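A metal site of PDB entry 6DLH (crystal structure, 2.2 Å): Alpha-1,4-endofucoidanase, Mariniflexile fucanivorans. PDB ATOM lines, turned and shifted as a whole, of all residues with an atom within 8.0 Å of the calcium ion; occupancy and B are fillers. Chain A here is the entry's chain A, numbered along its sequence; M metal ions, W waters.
O of Asp 336 lies within hydrogen-bond range of NH1 of Arg 328, 2.9 Å away.
Along chain A the residues within 4 Å of the calcium ion span positions 327 to 336.
The calcium ion is bound by OD1 of Asp 336 (2.2 Å), O of Arg 332 (2.3 Å), OD1 of Asn 335 (2.3 Å), OD1 of Asp 330 (2.4 Å), O of Phe 327 (2.4 Å) and water W1 (2.4 Å).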
ATOM      1  N   SER A 283      14.233  -2.237 -22.513  1.00  0.00           N
ATOM      2  CA  SER A 283      15.608  -2.279 -22.046  1.00  0.00           C
ATOM      3  C   SER A 283      15.680  -2.479 -20.531  1.00  0.00           C
ATOM      4  O   SER A 283      14.812  -2.025 -19.781  1.00  0.00           O
ATOM      5  CB  SER A 283      16.343  -1.027 -22.454  1.00  0.00           C
ATOM      6  OG  SER A 283      17.741  -1.256 -22.447  1.00  0.00           O
ATOM      7  N   ALA A 326      19.437 -11.002 -23.308  1.00  0.00           N
ATOM      8  CA  ALA A 326      18.453 -10.073 -23.844  1.00  0.00           C
ATOM      9  C   ALA A 326      19.104  -8.861 -24.516  1.00  0.00           C
ATOM     10  O   ALA A 326      18.541  -8.338 -25.480  1.00  0.00           O
ATOM     11  CB  ALA A 326      17.501  -9.646 -22.764  1.00  0.00           C
ATOM     12  N   PHE A 327      20.240  -8.389 -23.997  1.00  0.00           N
ATOM     13  CA  PHE A 327      20.670  -7.041 -24.353  1.00  0.00           C
ATOM     14  C   PHE A 327      22.127  -6.998 -24.816  1.00  0.00           C
ATOM     15  O   PHE A 327      22.831  -6.043 -24.508  1.00  0.00           O
ATOM     16  CB  PHE A 327      20.369  -6.071 -23.206  1.00  0.00           C
ATOM     17  CG  PHE A 327      18.920  -6.040 -22.812  1.00  0.00           C
ATOM     18  CD1 PHE A 327      17.949  -5.598 -23.706  1.00  0.00           C
ATOM     19  CD2 PHE A 327      18.505  -6.493 -21.565  1.00  0.00           C
ATOM     20  CE1 PHE A 327      16.602  -5.587 -23.356  1.00  0.00           C
ATOM     21  CE2 PHE A 327      17.168  -6.481 -21.215  1.00  0.00           C
ATOM     22  CZ  PHE A 327      16.216  -6.017 -22.113  1.00  0.00           C
ATOM     23  N   ARG A 328      22.554  -7.991 -25.600  1.00  0.00           N
ATOM     24  CA  ARG A 328      23.913  -7.980 -26.118  1.00  0.00           C
ATOM     25  C   ARG A 328      23.969  -7.215 -27.442  1.00  0.00           C
ATOM     26  O   ARG A 328      24.898  -7.399 -28.219  1.00  0.00           O
ATOM     27  CB  ARG A 328      24.493  -9.398 -26.195  1.00  0.00           C
ATOM     28  CG  ARG A 328      25.546  -9.687 -25.137  1.00  0.00           C
ATOM     29  CD  ARG A 328      25.288 -10.814 -24.150  1.00  0.00           C
ATOM     30  NE  ARG A 328      26.152 -11.946 -24.420  1.00  0.00           N
ATOM     31  CZ  ARG A 328      26.694 -12.748 -23.508  1.00  0.00           C
ATOM     32  NH1 ARG A 328      26.487 -12.571 -22.217  1.00  0.00           N
ATOM     33  NH2 ARG A 328      27.456 -13.760 -23.899  1.00  0.00           N
ATOM     34  N   ASP A 329      23.000  -6.309 -27.645  1.00  0.00           N
ATOM     35  CA  ASP A 329      22.751  -5.703 -28.937  1.00  0.00           C
ATOM     36  C   ASP A 329      22.878  -4.179 -28.873  1.00  0.00           C
ATOM     37  O   ASP A 329      22.701  -3.507 -29.884  1.00  0.00           O
ATOM     38  CB  ASP A 329      21.394  -6.154 -29.505  1.00  0.00           C
ATOM     39  CG  ASP A 329      20.165  -5.696 -28.723  1.00  0.00           C
ATOM     40  OD1 ASP A 329      20.322  -5.292 -27.540  1.00  0.00           O
ATOM     41  OD2 ASP A 329      19.065  -5.746 -29.285  1.00  0.00           O
ATOM     42  N   ASP A 330      23.171  -3.634 -27.691  1.00  0.00           N
ATOM     43  CA  ASP A 330      23.199  -2.193 -27.518  1.00  0.00           C
ATOM     44  C   ASP A 330      24.629  -1.737 -27.176  1.00  0.00           C
ATOM     45  O   ASP A 330      25.588  -2.483 -27.372  1.00  0.00           O
ATOM     46  CB  ASP A 330      22.156  -1.733 -26.491  1.00  0.00           C
ATOM     47  CG  ASP A 330      22.381  -2.255 -25.089  1.00  0.00           C
ATOM     48  OD1 ASP A 330      23.412  -2.947 -24.870  1.00  0.00           O
ATOM     49  OD2 ASP A 330      21.537  -1.981 -24.213  1.00  0.00           O
ATOM     50  N   THR A 331      24.729  -0.516 -26.619  1.00  0.00           N
ATOM     51  CA  THR A 331      26.014   0.120 -26.383  1.00  0.00           C
ATOM     52  C   THR A 331      26.391   0.092 -24.898  1.00  0.00           C
ATOM     53  O   THR A 331      27.460   0.567 -24.536  1.00  0.00           O
ATOM     54  CB  THR A 331      26.045   1.549 -26.968  1.00  0.00           C
ATOM     55  OG1 THR A 331      24.960   2.301 -26.430  1.00  0.00           O
ATOM     56  CG2 THR A 331      25.979   1.577 -28.478  1.00  0.00           C
ATOM     57  N   ARG A 332      25.516  -0.467 -24.056  1.00  0.00           N
ATOM     58  CA  ARG A 332      25.776  -0.571 -22.618  1.00  0.00           C
ATOM     59  C   ARG A 332      26.349  -1.956 -22.305  1.00  0.00           C
ATOM     60  O   ARG A 332      25.810  -2.967 -22.740  1.00  0.00           O
ATOM     61  CB  ARG A 332      24.484  -0.316 -21.836  1.00  0.00           C
ATOM     62  CG  ARG A 332      23.794   1.003 -22.166  1.00  0.00           C
ATOM     63  CD  ARG A 332      22.384   1.014 -21.617  1.00  0.00           C
ATOM     64  NE  ARG A 332      21.768   2.323 -21.534  1.00  0.00           N
ATOM     65  CZ  ARG A 332      20.599   2.580 -20.950  1.00  0.00           C
ATOM     66  NH1 ARG A 332      19.912   1.614 -20.367  1.00  0.00           N
ATOM     67  NH2 ARG A 332      20.126   3.817 -20.932  1.00  0.00           N
ATOM     68  N   THR A 333      27.448  -1.998 -21.535  1.00  0.00           N
ATOM     69  CA  THR A 333      28.107  -3.272 -21.227  1.00  0.00           C
ATOM     70  C   THR A 333      27.479  -3.917 -19.994  1.00  0.00           C
ATOM     71  O   THR A 333      27.537  -5.136 -19.829  1.00  0.00           O
ATOM     72  CB  THR A 333      29.597  -3.093 -20.936  1.00  0.00           C
ATOM     73  OG1 THR A 333      29.729  -2.170 -19.847  1.00  0.00           O
ATOM     74  CG2 THR A 333      30.402  -2.632 -22.135  1.00  0.00           C
ATOM     75  N   TRP A 334      26.906  -3.098 -19.120  1.00  0.00           N
ATOM     76  CA  TRP A 334      26.560  -3.554 -17.780  1.00  0.00           C
ATOM     77  C   TRP A 334      25.351  -4.495 -17.792  1.00  0.00           C
ATOM     78  O   TRP A 334      25.087  -5.154 -16.785  1.00  0.00           O
ATOM     79  CB  TRP A 334      26.334  -2.343 -16.863  1.00  0.00           C
ATOM     80  CG  TRP A 334      25.397  -1.325 -17.415  1.00  0.00           C
ATOM     81  CD1 TRP A 334      25.721  -0.191 -18.116  1.00  0.00           C
ATOM     82  CD2 TRP A 334      23.955  -1.326 -17.311  1.00  0.00           C
ATOM     83  NE1 TRP A 334      24.591   0.504 -18.442  1.00  0.00           N
ATOM     84  CE2 TRP A 334      23.496  -0.169 -17.974  1.00  0.00           C
ATOM     85  CE3 TRP A 334      23.014  -2.188 -16.731  1.00  0.00           C
ATOM     86  CZ2 TRP A 334      22.136   0.150 -18.062  1.00  0.00           C
ATOM     87  CZ3 TRP A 334      21.674  -1.873 -16.826  1.00  0.00           C
ATOM     88  CH2 TRP A 334      21.245  -0.723 -17.483  1.00  0.00           C
ATOM     89  N   ASN A 335      24.631  -4.548 -18.928  1.00  0.00           N
ATOM     90  CA  ASN A 335      23.376  -5.289 -19.006  1.00  0.00           C
ATOM     91  C   ASN A 335      23.563  -6.575 -19.805  1.00  0.00           C
ATOM     92  O   ASN A 335      22.590  -7.170 -20.260  1.00  0.00           O
ATOM     93  CB  ASN A 335      22.235  -4.428 -19.560  1.00  0.00           C
ATOM     94  CG  ASN A 335      22.413  -3.979 -21.003  1.00  0.00           C
ATOM     95  OD1 ASN A 335      23.263  -4.485 -21.739  1.00  0.00           O
ATOM     96  ND2 ASN A 335      21.607  -3.017 -21.419  1.00  0.00           N
ATOM     97  N   ASP A 336      24.821  -7.016 -19.956  1.00  0.00           N
ATOM     98  CA  ASP A 336      25.162  -8.046 -20.918  1.00  0.00           C
ATOM     99  C   ASP A 336      24.860  -9.442 -20.381  1.00  0.00           C
ATOM    100  O   ASP A 336      24.956 -10.408 -21.138  1.00  0.00           O
ATOM    101  CB  ASP A 336      26.617  -7.931 -21.385  1.00  0.00           C
ATOM    102  CG  ASP A 336      26.823  -6.969 -22.538  1.00  0.00           C
ATOM    103  OD1 ASP A 336      25.872  -6.216 -22.876  1.00  0.00           O
ATOM    104  OD2 ASP A 336      27.933  -6.969 -23.096  1.00  0.00           O
ATOM    105  N   ASN A 337      24.523  -9.562 -19.096  1.00  0.00           N
ATOM    106  CA  ASN A 337      24.228 -10.864 -18.518  1.00  0.00           C
ATOM    107  C   ASN A 337      22.746 -10.997 -18.189  1.00  0.00           C
ATOM    108  O   ASN A 337      22.324 -12.052 -17.729  1.00  0.00           O
ATOM    109  CB  ASN A 337      25.090 -11.196 -17.297  1.00  0.00           C
ATOM    110  CG  ASN A 337      26.570 -11.283 -17.634  1.00  0.00           C
ATOM    111  OD1 ASN A 337      27.387 -10.609 -17.006  1.00  0.00           O
ATOM    112  ND2 ASN A 337      26.913 -12.095 -18.623  1.00  0.00           N
ATOM    113  N   VAL A 338      21.964  -9.935 -18.441  1.00  0.00           N
ATOM    114  CA  VAL A 338      20.521  -9.968 -18.262  1.00  0.00           C
ATOM    115  C   VAL A 338      19.932 -11.078 -19.139  1.00  0.00           C
ATOM    116  O   VAL A 338      20.276 -11.201 -20.314  1.00  0.00           O
ATOM    117  CB  VAL A 338      19.908  -8.584 -18.526  1.00  0.00           C
ATOM    118  CG1 VAL A 338      18.387  -8.601 -18.489  1.00  0.00           C
ATOM    119  CG2 VAL A 338      20.447  -7.537 -17.566  1.00  0.00           C
HETATM  120 CA    CA M   1      24.529  -4.617 -23.612  1.00  0.00          CA
HETATM  121  O   HOH W   1      25.753  -4.884 -25.709  1.00  0.00           O
